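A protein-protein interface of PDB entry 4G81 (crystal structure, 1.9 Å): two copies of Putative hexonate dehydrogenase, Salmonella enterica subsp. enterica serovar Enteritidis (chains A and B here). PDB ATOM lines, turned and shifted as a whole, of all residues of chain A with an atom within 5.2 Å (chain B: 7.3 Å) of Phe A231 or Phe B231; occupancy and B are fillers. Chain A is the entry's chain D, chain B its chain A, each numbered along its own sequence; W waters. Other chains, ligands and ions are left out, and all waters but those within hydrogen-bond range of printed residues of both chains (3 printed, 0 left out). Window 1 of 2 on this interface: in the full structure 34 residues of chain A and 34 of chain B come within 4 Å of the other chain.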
ATOM      1  N   PHE A   5      31.781   6.049   8.625  1.00  0.00           N
ATOM      2  CA  PHE A   5      31.981   6.954   7.497  1.00  0.00           C
ATOM      3  C   PHE A   5      32.545   8.308   7.920  1.00  0.00           C
ATOM      4  O   PHE A   5      32.563   9.251   7.126  1.00  0.00           O
ATOM      5  CB  PHE A   5      30.664   7.142   6.721  1.00  0.00           C
ATOM      6  CG  PHE A   5      30.073   5.861   6.205  1.00  0.00           C
ATOM      7  CD1 PHE A   5      30.476   5.342   4.980  1.00  0.00           C
ATOM      8  CD2 PHE A   5      29.113   5.174   6.940  1.00  0.00           C
ATOM      9  CE1 PHE A   5      29.929   4.159   4.490  1.00  0.00           C
ATOM     10  CE2 PHE A   5      28.562   3.976   6.455  1.00  0.00           C
ATOM     11  CZ  PHE A   5      28.973   3.475   5.228  1.00  0.00           C
ATOM     12  N   ILE A 226      29.460  12.493  -4.033  1.00  0.00           N
ATOM     13  CA  ILE A 226      30.078  12.676  -2.717  1.00  0.00           C
ATOM     14  C   ILE A 226      30.020  11.419  -1.842  1.00  0.00           C
ATOM     15  O   ILE A 226      30.999  11.087  -1.158  1.00  0.00           O
ATOM     16  CB  ILE A 226      29.453  13.889  -1.995  1.00  0.00           C
ATOM     17  CG1 ILE A 226      29.984  15.182  -2.615  1.00  0.00           C
ATOM     18  CG2 ILE A 226      29.736  13.856  -0.500  1.00  0.00           C
ATOM     19  CD1 ILE A 226      29.312  16.456  -2.085  1.00  0.00           C
ATOM     20  N   GLY A 227      28.884  10.718  -1.864  1.00  0.00           N
ATOM     21  CA  GLY A 227      28.732   9.487  -1.096  1.00  0.00           C
ATOM     22  C   GLY A 227      29.803   8.455  -1.408  1.00  0.00           C
ATOM     23  O   GLY A 227      30.366   7.819  -0.508  1.00  0.00           O
ATOM     24  N   THR A 228      30.091   8.288  -2.692  1.00  0.00           N
ATOM     25  CA  THR A 228      31.103   7.328  -3.131  1.00  0.00           C
ATOM     26  C   THR A 228      32.487   7.770  -2.663  1.00  0.00           C
ATOM     27  O   THR A 228      33.301   6.943  -2.223  1.00  0.00           O
ATOM     28  CB  THR A 228      31.088   7.197  -4.658  1.00  0.00           C
ATOM     29  OG1 THR A 228      29.776   6.786  -5.085  1.00  0.00           O
ATOM     30  CG2 THR A 228      32.126   6.174  -5.143  1.00  0.00           C
ATOM     31  N   ALA A 229      32.758   9.070  -2.747  1.00  0.00           N
ATOM     32  CA  ALA A 229      34.068   9.584  -2.345  1.00  0.00           C
ATOM     33  C   ALA A 229      34.304   9.340  -0.853  1.00  0.00           C
ATOM     34  O   ALA A 229      35.384   8.911  -0.444  1.00  0.00           O
ATOM     35  CB  ALA A 229      34.212  11.076  -2.696  1.00  0.00           C
ATOM     36  N   ILE A 230      33.289   9.612  -0.041  1.00  0.00           N
ATOM     37  CA  ILE A 230      33.409   9.400   1.398  1.00  0.00           C
ATOM     38  C   ILE A 230      33.550   7.913   1.712  1.00  0.00           C
ATOM     39  O   ILE A 230      34.395   7.526   2.518  1.00  0.00           O
ATOM     40  CB  ILE A 230      32.195   9.965   2.139  1.00  0.00           C
ATOM     41  CG1 ILE A 230      32.116  11.476   1.948  1.00  0.00           C
ATOM     42  CG2 ILE A 230      32.236   9.588   3.623  1.00  0.00           C
ATOM     43  CD1 ILE A 230      30.761  12.051   2.360  1.00  0.00           C
ATOM     44  N   PHE A 231      32.712   7.096   1.073  1.00  0.00           N
ATOM     45  CA  PHE A 231      32.762   5.636   1.169  1.00  0.00           C
ATOM     46  C   PHE A 231      34.187   5.145   0.928  1.00  0.00           C
ATOM     47  O   PHE A 231      34.770   4.476   1.790  1.00  0.00           O
ATOM     48  CB  PHE A 231      31.770   5.038   0.158  1.00  0.00           C
ATOM     49  CG  PHE A 231      31.833   3.537   0.015  1.00  0.00           C
ATOM     50  CD1 PHE A 231      31.600   2.695   1.099  1.00  0.00           C
ATOM     51  CD2 PHE A 231      32.068   2.967  -1.233  1.00  0.00           C
ATOM     52  CE1 PHE A 231      31.647   1.298   0.936  1.00  0.00           C
ATOM     53  CE2 PHE A 231      32.110   1.584  -1.402  1.00  0.00           C
ATOM     54  CZ  PHE A 231      31.892   0.749  -0.327  1.00  0.00           C
ATOM     55  N   LEU A 232      34.761   5.512  -0.216  1.00  0.00           N
ATOM     56  CA  LEU A 232      36.103   5.067  -0.570  1.00  0.00           C
ATOM     57  C   LEU A 232      37.213   5.726   0.242  1.00  0.00           C
ATOM     58  O   LEU A 232      38.363   5.284   0.174  1.00  0.00           O
ATOM     59  CB  LEU A 232      36.378   5.249  -2.073  1.00  0.00           C
ATOM     60  CG  LEU A 232      35.531   4.401  -3.019  1.00  0.00           C
ATOM     61  CD1 LEU A 232      35.901   4.688  -4.481  1.00  0.00           C
ATOM     62  CD2 LEU A 232      35.669   2.905  -2.708  1.00  0.00           C
ATOM     63  N   SER A 233      36.889   6.763   1.015  1.00  0.00           N
ATOM     64  CA  SER A 233      37.895   7.443   1.835  1.00  0.00           C
ATOM     65  C   SER A 233      37.837   6.987   3.285  1.00  0.00           C
ATOM     66  O   SER A 233      38.657   7.402   4.104  1.00  0.00           O
ATOM     67  CB  SER A 233      37.698   8.966   1.809  1.00  0.00           C
ATOM     68  OG  SER A 233      37.836   9.490   0.500  1.00  0.00           O
ATOM     69  N   SER A 234      36.862   6.147   3.607  1.00  0.00           N
ATOM     70  CA  SER A 234      36.563   5.849   5.005  1.00  0.00           C
ATOM     71  C   SER A 234      36.848   4.398   5.374  1.00  0.00           C
ATOM     72  O   SER A 234      37.178   3.577   4.519  1.00  0.00           O
ATOM     73  CB  SER A 234      35.091   6.146   5.289  1.00  0.00           C
ATOM     74  OG  SER A 234      34.284   5.178   4.639  1.00  0.00           O
ATOM     75  N   ALA A 236      34.840   2.210   5.890  1.00  0.00           N
ATOM     76  CA  ALA A 236      33.888   1.372   5.171  1.00  0.00           C
ATOM     77  C   ALA A 236      34.519   0.636   3.992  1.00  0.00           C
ATOM     78  O   ALA A 236      33.999  -0.383   3.541  1.00  0.00           O
ATOM     79  CB  ALA A 236      32.711   2.208   4.705  1.00  0.00           C
ATOM     80  N   SER A 237      35.634   1.149   3.477  1.00  0.00           N
ATOM     81  CA  SER A 237      36.269   0.543   2.309  1.00  0.00           C
ATOM     82  C   SER A 237      37.625  -0.097   2.635  1.00  0.00           C
ATOM     83  O   SER A 237      38.456  -0.302   1.741  1.00  0.00           O
ATOM     84  CB  SER A 237      36.445   1.596   1.214  1.00  0.00           C
ATOM     85  OG  SER A 237      37.237   2.672   1.691  1.00  0.00           O
ATOM     86  N   ILE A 240      38.284  -3.025   0.445  1.00  0.00           N
ATOM     87  CA  ILE A 240      38.033  -2.801  -0.987  1.00  0.00           C
ATOM     88  C   ILE A 240      39.303  -2.274  -1.615  1.00  0.00           C
ATOM     89  O   ILE A 240      39.923  -1.343  -1.095  1.00  0.00           O
ATOM     90  CB  ILE A 240      36.886  -1.793  -1.219  1.00  0.00           C
ATOM     91  CG1 ILE A 240      35.651  -2.252  -0.462  1.00  0.00           C
ATOM     92  CG2 ILE A 240      36.541  -1.678  -2.706  1.00  0.00           C
ATOM     93  CD1 ILE A 240      34.451  -1.365  -0.695  1.00  0.00           C
ATOM     94  N   ILE A 245      34.021   2.156  -9.196  1.00  0.00           N
ATOM     95  CA  ILE A 245      32.598   2.233  -8.965  1.00  0.00           C
ATOM     96  C   ILE A 245      32.043   3.263  -9.931  1.00  0.00           C
ATOM     97  O   ILE A 245      32.433   4.432  -9.884  1.00  0.00           O
ATOM     98  CB  ILE A 245      32.309   2.634  -7.493  1.00  0.00           C
ATOM     99  CG1 ILE A 245      32.795   1.537  -6.529  1.00  0.00           C
ATOM    100  CG2 ILE A 245      30.825   2.873  -7.289  1.00  0.00           C
ATOM    101  CD1 ILE A 245      32.852   1.998  -5.052  1.00  0.00           C
ATOM    102  N   LEU B   4      23.687  11.515   4.844  1.00  0.00           N
ATOM    103  CA  LEU B   4      23.954  10.700   3.659  1.00  0.00           C
ATOM    104  C   LEU B   4      23.826   9.188   3.847  1.00  0.00           C
ATOM    105  O   LEU B   4      23.321   8.486   2.967  1.00  0.00           O
ATOM    106  CB  LEU B   4      25.358  10.991   3.129  1.00  0.00           C
ATOM    107  CG  LEU B   4      25.492  11.664   1.769  1.00  0.00           C
ATOM    108  CD1 LEU B   4      26.922  11.546   1.243  1.00  0.00           C
ATOM    109  CD2 LEU B   4      24.503  11.106   0.775  1.00  0.00           C
ATOM    110  N   PHE B   5      24.323   8.684   4.971  1.00  0.00           N
ATOM    111  CA  PHE B   5      24.397   7.243   5.190  1.00  0.00           C
ATOM    112  C   PHE B   5      23.437   6.760   6.282  1.00  0.00           C
ATOM    113  O   PHE B   5      23.508   5.605   6.719  1.00  0.00           O
ATOM    114  CB  PHE B   5      25.828   6.854   5.569  1.00  0.00           C
ATOM    115  CG  PHE B   5      26.844   7.160   4.502  1.00  0.00           C
ATOM    116  CD1 PHE B   5      27.104   6.239   3.498  1.00  0.00           C
ATOM    117  CD2 PHE B   5      27.536   8.363   4.502  1.00  0.00           C
ATOM    118  CE1 PHE B   5      28.046   6.502   2.508  1.00  0.00           C
ATOM    119  CE2 PHE B   5      28.482   8.641   3.511  1.00  0.00           C
ATOM    120  CZ  PHE B   5      28.737   7.707   2.512  1.00  0.00           C
ATOM    121  N   LEU B   7      20.094   5.437   7.813  1.00  0.00           N
ATOM    122  CA  LEU B   7      18.979   4.588   7.385  1.00  0.00           C
ATOM    123  C   LEU B   7      17.772   4.698   8.325  1.00  0.00           C
ATOM    124  O   LEU B   7      16.851   3.885   8.262  1.00  0.00           O
ATOM    125  CB  LEU B   7      19.428   3.128   7.317  1.00  0.00           C
ATOM    126  CG  LEU B   7      20.565   2.853   6.328  1.00  0.00           C
ATOM    127  CD1 LEU B   7      20.921   1.364   6.272  1.00  0.00           C
ATOM    128  CD2 LEU B   7      20.208   3.381   4.936  1.00  0.00           C
ATOM    129  N   LEU B  29      22.860  -2.909   9.099  1.00  0.00           N
ATOM    130  CA  LEU B  29      21.822  -1.971   8.682  1.00  0.00           C
ATOM    131  C   LEU B  29      21.085  -1.415   9.900  1.00  0.00           C
ATOM    132  O   LEU B  29      20.731  -0.224   9.938  1.00  0.00           O
ATOM    133  CB  LEU B  29      20.830  -2.636   7.725  1.00  0.00           C
ATOM    134  CG  LEU B  29      21.327  -3.155   6.376  1.00  0.00           C
ATOM    135  CD1 LEU B  29      20.177  -3.779   5.590  1.00  0.00           C
ATOM    136  CD2 LEU B  29      21.994  -2.055   5.555  1.00  0.00           C
ATOM    137  N   LYS B 140      15.740   0.271  -2.459  1.00  0.00           N
ATOM    138  CA  LYS B 140      17.089  -0.213  -2.685  1.00  0.00           C
ATOM    139  C   LYS B 140      17.030  -1.731  -2.725  1.00  0.00           C
ATOM    140  O   LYS B 140      16.408  -2.359  -1.856  1.00  0.00           O
ATOM    141  CB  LYS B 140      18.011   0.221  -1.539  1.00  0.00           C
ATOM    142  CG  LYS B 140      18.044   1.727  -1.274  1.00  0.00           C
ATOM    143  CD  LYS B 140      18.801   2.445  -2.395  1.00  0.00           C
ATOM    144  CE  LYS B 140      19.074   3.903  -2.046  1.00  0.00           C
ATOM    145  NZ  LYS B 140      20.037   4.486  -3.021  1.00  0.00           N
ATOM    146  N   ILE B 142      19.691  -4.996  -3.049  1.00  0.00           N
ATOM    147  CA  ILE B 142      21.070  -5.427  -3.115  1.00  0.00           C
ATOM    148  C   ILE B 142      21.139  -6.935  -3.297  1.00  0.00           C
ATOM    149  O   ILE B 142      20.725  -7.700  -2.417  1.00  0.00           O
ATOM    150  CB  ILE B 142      21.843  -5.054  -1.845  1.00  0.00           C
ATOM    151  CG1 ILE B 142      21.824  -3.538  -1.628  1.00  0.00           C
ATOM    152  CG2 ILE B 142      23.277  -5.527  -1.956  1.00  0.00           C
ATOM    153  CD1 ILE B 142      22.470  -3.107  -0.322  1.00  0.00           C
ATOM    154  N   ASN B 185      21.741  -2.834  -6.950  1.00  0.00           N
ATOM    155  CA  ASN B 185      23.166  -3.091  -7.090  1.00  0.00           C
ATOM    156  C   ASN B 185      23.527  -4.406  -6.410  1.00  0.00           C
ATOM    157  O   ASN B 185      22.652  -5.094  -5.880  1.00  0.00           O
ATOM    158  CB  ASN B 185      23.949  -1.929  -6.494  1.00  0.00           C
ATOM    159  CG  ASN B 185      23.692  -0.635  -7.235  1.00  0.00           C
ATOM    160  OD1 ASN B 185      24.196  -0.434  -8.343  1.00  0.00           O
ATOM    161  ND2 ASN B 185      22.903   0.246  -6.634  1.00  0.00           N
ATOM    162  N   GLU B 224      33.443  -6.055   7.602  1.00  0.00           N
ATOM    163  CA  GLU B 224      34.042  -5.256   6.544  1.00  0.00           C
ATOM    164  C   GLU B 224      33.156  -5.203   5.318  1.00  0.00           C
ATOM    165  O   GLU B 224      33.492  -4.551   4.324  1.00  0.00           O
ATOM    166  CB  GLU B 224      35.423  -5.794   6.196  1.00  0.00           C
ATOM    167  CG  GLU B 224      36.334  -5.849   7.411  1.00  0.00           C
ATOM    168  CD  GLU B 224      37.764  -6.109   7.042  1.00  0.00           C
ATOM    169  OE1 GLU B 224      38.105  -7.293   6.833  1.00  0.00           O
ATOM    170  OE2 GLU B 224      38.546  -5.134   6.953  1.00  0.00           O
ATOM    171  N   LEU B 225      32.024  -5.901   5.379  1.00  0.00           N
ATOM    172  CA  LEU B 225      31.024  -5.814   4.312  1.00  0.00           C
ATOM    173  C   LEU B 225      29.903  -4.814   4.626  1.00  0.00           C
ATOM    174  O   LEU B 225      29.146  -4.417   3.731  1.00  0.00           O
ATOM    175  CB  LEU B 225      30.424  -7.193   4.020  1.00  0.00           C
ATOM    176  CG  LEU B 225      31.393  -8.277   3.552  1.00  0.00           C
ATOM    177  CD1 LEU B 225      30.773  -9.641   3.780  1.00  0.00           C
ATOM    178  CD2 LEU B 225      31.717  -8.099   2.084  1.00  0.00           C
ATOM    179  N   ILE B 226      29.800  -4.420   5.893  1.00  0.00           N
ATOM    180  CA  ILE B 226      28.727  -3.552   6.389  1.00  0.00           C
ATOM    181  C   ILE B 226      28.690  -2.186   5.712  1.00  0.00           C
ATOM    182  O   ILE B 226      27.619  -1.687   5.347  1.00  0.00           O
ATOM    183  CB  ILE B 226      28.879  -3.313   7.914  1.00  0.00           C
ATOM    184  CG1 ILE B 226      28.790  -4.635   8.662  1.00  0.00           C
ATOM    185  CG2 ILE B 226      27.815  -2.364   8.429  1.00  0.00           C
ATOM    186  CD1 ILE B 226      27.737  -5.539   8.105  1.00  0.00           C
ATOM    187  N   GLY B 227      29.860  -1.572   5.565  1.00  0.00           N
ATOM    188  CA  GLY B 227      29.934  -0.265   4.940  1.00  0.00           C
ATOM    189  C   GLY B 227      29.342  -0.283   3.541  1.00  0.00           C
ATOM    190  O   GLY B 227      28.615   0.642   3.157  1.00  0.00           O
ATOM    191  N   THR B 228      29.626  -1.345   2.785  1.00  0.00           N
ATOM    192  CA  THR B 228      29.122  -1.437   1.418  1.00  0.00           C
ATOM    193  C   THR B 228      27.612  -1.641   1.418  1.00  0.00           C
ATOM    194  O   THR B 228      26.912  -1.065   0.593  1.00  0.00           O
ATOM    195  CB  THR B 228      29.800  -2.584   0.621  1.00  0.00           C
ATOM    196  OG1 THR B 228      31.221  -2.402   0.639  1.00  0.00           O
ATOM    197  CG2 THR B 228      29.338  -2.586  -0.838  1.00  0.00           C
ATOM    198  N   ALA B 229      27.107  -2.465   2.333  1.00  0.00           N
ATOM    199  CA  ALA B 229      25.654  -2.650   2.462  1.00  0.00           C
ATOM    200  C   ALA B 229      24.934  -1.332   2.776  1.00  0.00           C
ATOM    201  O   ALA B 229      23.930  -0.980   2.147  1.00  0.00           O
ATOM    202  CB  ALA B 229      25.335  -3.691   3.548  1.00  0.00           C
ATOM    203  N   ILE B 230      25.427  -0.618   3.777  1.00  0.00           N
ATOM    204  CA  ILE B 230      24.839   0.670   4.148  1.00  0.00           C
ATOM    205  C   ILE B 230      24.890   1.679   2.986  1.00  0.00           C
ATOM    206  O   ILE B 230      23.898   2.370   2.680  1.00  0.00           O
ATOM    207  CB  ILE B 230      25.574   1.253   5.353  1.00  0.00           C
ATOM    208  CG1 ILE B 230      25.360   0.358   6.573  1.00  0.00           C
ATOM    209  CG2 ILE B 230      25.058   2.656   5.663  1.00  0.00           C
ATOM    210  CD1 ILE B 230      26.239   0.748   7.743  1.00  0.00           C
ATOM    211  N   PHE B 231      26.056   1.763   2.361  1.00  0.00           N
ATOM    212  CA  PHE B 231      26.291   2.605   1.189  1.00  0.00           C
ATOM    213  C   PHE B 231      25.222   2.358   0.120  1.00  0.00           C
ATOM    214  O   PHE B 231      24.523   3.275  -0.319  1.00  0.00           O
ATOM    215  CB  PHE B 231      27.688   2.283   0.652  1.00  0.00           C
ATOM    216  CG  PHE B 231      28.037   2.970  -0.652  1.00  0.00           C
ATOM    217  CD1 PHE B 231      27.992   4.362  -0.766  1.00  0.00           C
ATOM    218  CD2 PHE B 231      28.449   2.220  -1.749  1.00  0.00           C
ATOM    219  CE1 PHE B 231      28.333   4.987  -1.973  1.00  0.00           C
ATOM    220  CE2 PHE B 231      28.793   2.836  -2.963  1.00  0.00           C
ATOM    221  CZ  PHE B 231      28.735   4.220  -3.069  1.00  0.00           C
ATOM    222  N   LEU B 232      25.063   1.099  -0.263  1.00  0.00           N
ATOM    223  CA  LEU B 232      24.098   0.745  -1.291  1.00  0.00           C
ATOM    224  C   LEU B 232      22.650   0.749  -0.790  1.00  0.00           C
ATOM    225  O   LEU B 232      21.726   0.575  -1.584  1.00  0.00           O
ATOM    226  CB  LEU B 232      24.472  -0.604  -1.922  1.00  0.00           C
ATOM    227  CG  LEU B 232      25.796  -0.648  -2.675  1.00  0.00           C
ATOM    228  CD1 LEU B 232      26.143  -2.094  -3.025  1.00  0.00           C
ATOM    229  CD2 LEU B 232      25.715   0.200  -3.945  1.00  0.00           C
ATOM    230  N   SER B 233      22.440   0.962   0.511  1.00  0.00           N
ATOM    231  CA  SER B 233      21.082   1.059   1.047  1.00  0.00           C
ATOM    232  C   SER B 233      20.651   2.503   1.306  1.00  0.00           C
ATOM    233  O   SER B 233      19.510   2.743   1.701  1.00  0.00           O
ATOM    234  CB  SER B 233      20.962   0.293   2.373  1.00  0.00           C
ATOM    235  OG  SER B 233      21.205  -1.086   2.199  1.00  0.00           O
ATOM    236  N   SER B 234      21.557   3.454   1.116  1.00  0.00           N
ATOM    237  CA  SER B 234      21.323   4.819   1.589  1.00  0.00           C
ATOM    238  C   SER B 234      21.306   5.834   0.449  1.00  0.00           C
ATOM    239  O   SER B 234      21.535   5.480  -0.710  1.00  0.00           O
ATOM    240  CB  SER B 234      22.402   5.220   2.583  1.00  0.00           C
ATOM    241  OG  SER B 234      23.641   5.283   1.909  1.00  0.00           O
ATOM    242  N   LYS B 235      21.068   7.101   0.793  1.00  0.00           N
ATOM    243  CA  LYS B 235      21.017   8.178  -0.201  1.00  0.00           C
ATOM    244  C   LYS B 235      22.335   8.319  -0.940  1.00  0.00           C
ATOM    245  O   LYS B 235      22.386   8.832  -2.061  1.00  0.00           O
ATOM    246  CB  LYS B 235      20.643   9.516   0.469  1.00  0.00           C
ATOM    247  CG  LYS B 235      19.234   9.545   1.036  1.00  0.00           C
ATOM    248  CD  LYS B 235      18.878  10.924   1.588  1.00  0.00           C
ATOM    249  CE  LYS B 235      19.424  11.132   2.999  1.00  0.00           C
ATOM    250  NZ  LYS B 235      18.760  10.246   3.997  1.00  0.00           N
ATOM    251  N   ALA B 236      23.409   7.854  -0.307  1.00  0.00           N
ATOM    252  CA  ALA B 236      24.741   7.913  -0.895  1.00  0.00           C
ATOM    253  C   ALA B 236      24.852   7.204  -2.252  1.00  0.00           C
ATOM    254  O   ALA B 236      25.779   7.470  -3.021  1.00  0.00           O
ATOM    255  CB  ALA B 236      25.755   7.356   0.078  1.00  0.00           C
ATOM    256  N   SER B 237      23.917   6.299  -2.543  1.00  0.00           N
ATOM    257  CA  SER B 237      23.960   5.521  -3.775  1.00  0.00           C
ATOM    258  C   SER B 237      22.774   5.800  -4.704  1.00  0.00           C
ATOM    259  O   SER B 237      22.452   4.979  -5.566  1.00  0.00           O
ATOM    260  CB  SER B 237      24.021   4.020  -3.461  1.00  0.00           C
ATOM    261  OG  SER B 237      22.927   3.622  -2.642  1.00  0.00           O
ATOM    262  N   ASP B 238      22.134   6.954  -4.544  1.00  0.00           N
ATOM    263  CA  ASP B 238      20.938   7.276  -5.336  1.00  0.00           C
ATOM    264  C   ASP B 238      21.156   7.281  -6.861  1.00  0.00           C
ATOM    265  O   ASP B 238      20.235   6.977  -7.620  1.00  0.00           O
ATOM    266  CB  ASP B 238      20.330   8.602  -4.873  1.00  0.00           C
ATOM    267  CG  ASP B 238      19.443   8.446  -3.631  1.00  0.00           C
ATOM    268  OD1 ASP B 238      19.398   7.338  -3.040  1.00  0.00           O
ATOM    269  OD2 ASP B 238      18.785   9.441  -3.258  1.00  0.00           O
ATOM    270  N   ILE B 240      23.565   5.381  -8.319  1.00  0.00           N
ATOM    271  CA  ILE B 240      24.293   4.150  -8.653  1.00  0.00           C
ATOM    272  C   ILE B 240      23.270   3.058  -8.940  1.00  0.00           C
ATOM    273  O   ILE B 240      22.355   2.820  -8.143  1.00  0.00           O
ATOM    274  CB  ILE B 240      25.230   3.723  -7.495  1.00  0.00           C
ATOM    275  CG1 ILE B 240      26.213   4.850  -7.178  1.00  0.00           C
ATOM    276  CG2 ILE B 240      25.995   2.465  -7.834  1.00  0.00           C
ATOM    277  CD1 ILE B 240      27.030   4.600  -5.935  1.00  0.00           C
ATOM    278  N   ILE B 245      29.922  -4.386  -6.590  1.00  0.00           N
ATOM    279  CA  ILE B 245      31.090  -3.906  -5.867  1.00  0.00           C
ATOM    280  C   ILE B 245      31.730  -5.109  -5.191  1.00  0.00           C
ATOM    281  O   ILE B 245      31.101  -5.760  -4.360  1.00  0.00           O
ATOM    282  CB  ILE B 245      30.671  -2.843  -4.821  1.00  0.00           C
ATOM    283  CG1 ILE B 245      30.116  -1.599  -5.537  1.00  0.00           C
ATOM    284  CG2 ILE B 245      31.847  -2.476  -3.906  1.00  0.00           C
ATOM    285  CD1 ILE B 245      29.571  -0.547  -4.599  1.00  0.00           C
ATOM    286  N   VAL B 247      34.289  -6.849  -2.641  1.00  0.00           N
ATOM    287  CA  VAL B 247      34.931  -6.533  -1.373  1.00  0.00           C
ATOM    288  C   VAL B 247      35.860  -7.698  -1.080  1.00  0.00           C
ATOM    289  O   VAL B 247      35.484  -8.662  -0.419  1.00  0.00           O
ATOM    290  CB  VAL B 247      33.876  -6.312  -0.274  1.00  0.00           C
ATOM    291  CG1 VAL B 247      34.528  -5.860   1.038  1.00  0.00           C
ATOM    292  CG2 VAL B 247      32.873  -5.259  -0.727  1.00  0.00           C
HETATM  293  O   HOH W   1      27.835   8.631  -4.409  1.00  0.00           O
HETATM  294  O   HOH W   2      32.310  -2.498   3.134  1.00  0.00           O
HETATM  295  O   HOH W   3      35.678  -3.001   3.593  1.00  0.00           O
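OG of Ser A234 lies within hydrogen-bond range of O of Ile A230 (3.2 Å).
O of Phe A231 sits at hydrogen-bond distance from OG of Ser A234 (3.0 Å).
The side-chain hydroxyl (OG) of Ser A234 lies close to the backbone NH (N) of Ala A236, at 3.3 Å.
O of Leu B4 is in hydrogen-bond range of OG of Ser B234.
O of Ile B230 is in hydrogen-bond range of OG of Ser B234.
The side-chain hydroxyl (OG) of Ser B237 is in hydrogen-bond range of the backbone carbonyl oxygen (O) of Phe B231 (2.8 Å).
Among the printed residues, pairs that only touch across the chains: Phe A5 with Phe B5 (3.6 Å), Phe A5 with Gly B227 (3.5 Å), Phe A5 with Ile B230 (3.8 Å), Gly A227 with Leu B4 (3.6 Å), Gly A227 with Phe B5 (3.4 Å), Gly A227 with Phe B231 (3.8 Å), Gly A227 with Ala B236 (3.8 Å), Thr A228 with Phe B231 (3.4 Å), Thr A228 with Ile B240 (3.6 Å), Ile A230 with Phe B5 (3.9 Å), Phe A231 with Gly B227 (3.8 Å), Phe A231 with Thr B228 (3.4 Å), Phe A231 with Phe B231 (3.7 Å), Ala A236 with Gly B227 (3.7 Å) and Ile A240 with Thr B228 (3.6 Å).
Of the printed residues of chain B, Ile A230 touches Phe B5 (3.9 Å).
Phe A231 touches just these residues of chain B: Gly B227 (3.8 Å), Thr B228 (3.4 Å) and Phe B231 (3.7 Å).
Of chain A, only Gly A227 (3.8 Å), Thr A228 (3.4 Å) and Phe A231 (3.7 Å) come within 4 Å of Phe B231.
Ser B234 touches none of the printed residues of chain A.
Ser B237 touches none of the printed residues of chain A.
Printed residues of chain A within 4 Å of Ile B240: Thr A228 (3.6 Å).
The nearest residue of chain B that does not touch Phe A231 is Phe B5 (4.3 Å).
The nearest printed residue of chain B that does not touch Phe A5 is Phe B231 (4.4 Å).
Of the 14 printed residues of chain A, 7 touch a printed residue of chain B.
Hydrophobic or aromatic side chains of chain A within 4 Å of the printed part of chain B: Phe A5, Ile A230, Phe A231, Ala A236 and Ile A240.
Along chain A the printed residues that touch a printed residue of chain B span positions 5 to 240.
Of the 25 printed residues of chain B, 8 touch a printed residue of chain A.
Among the printed residues, no Asp or Glu carboxylate lies within 4 Å of a Lys or Arg side-chain nitrogen of the other chain.
Phe A5 touches Gly B227, and with the chains exchanged Gly A227 touches Phe B5.
Phe A5 touches Ile B230, and with the chains exchanged Ile A230 touches Phe B5.
Thr A228 touches Ile B240, and with the chains exchanged Ile A240 touches Thr B228.
Phe A231 touches its own counterpart, Phe B231.
Water W2 lies within hydrogen-bond range of the backbone carbonyl oxygen of Glu B224, the side-chain hydroxyl of Thr B228 and the backbone carbonyl oxygen of Ala A236.
Water W1 lies within hydrogen-bond range of the backbone carbonyl oxygen of Ala B236, the side-chain hydroxyl of Thr A228 and the backbone NH of Gly A227.
Water W3 lies within hydrogen-bond range of the backbone carbonyl oxygen of Glu B224 and the backbone carbonyl oxygen of Ala A236.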
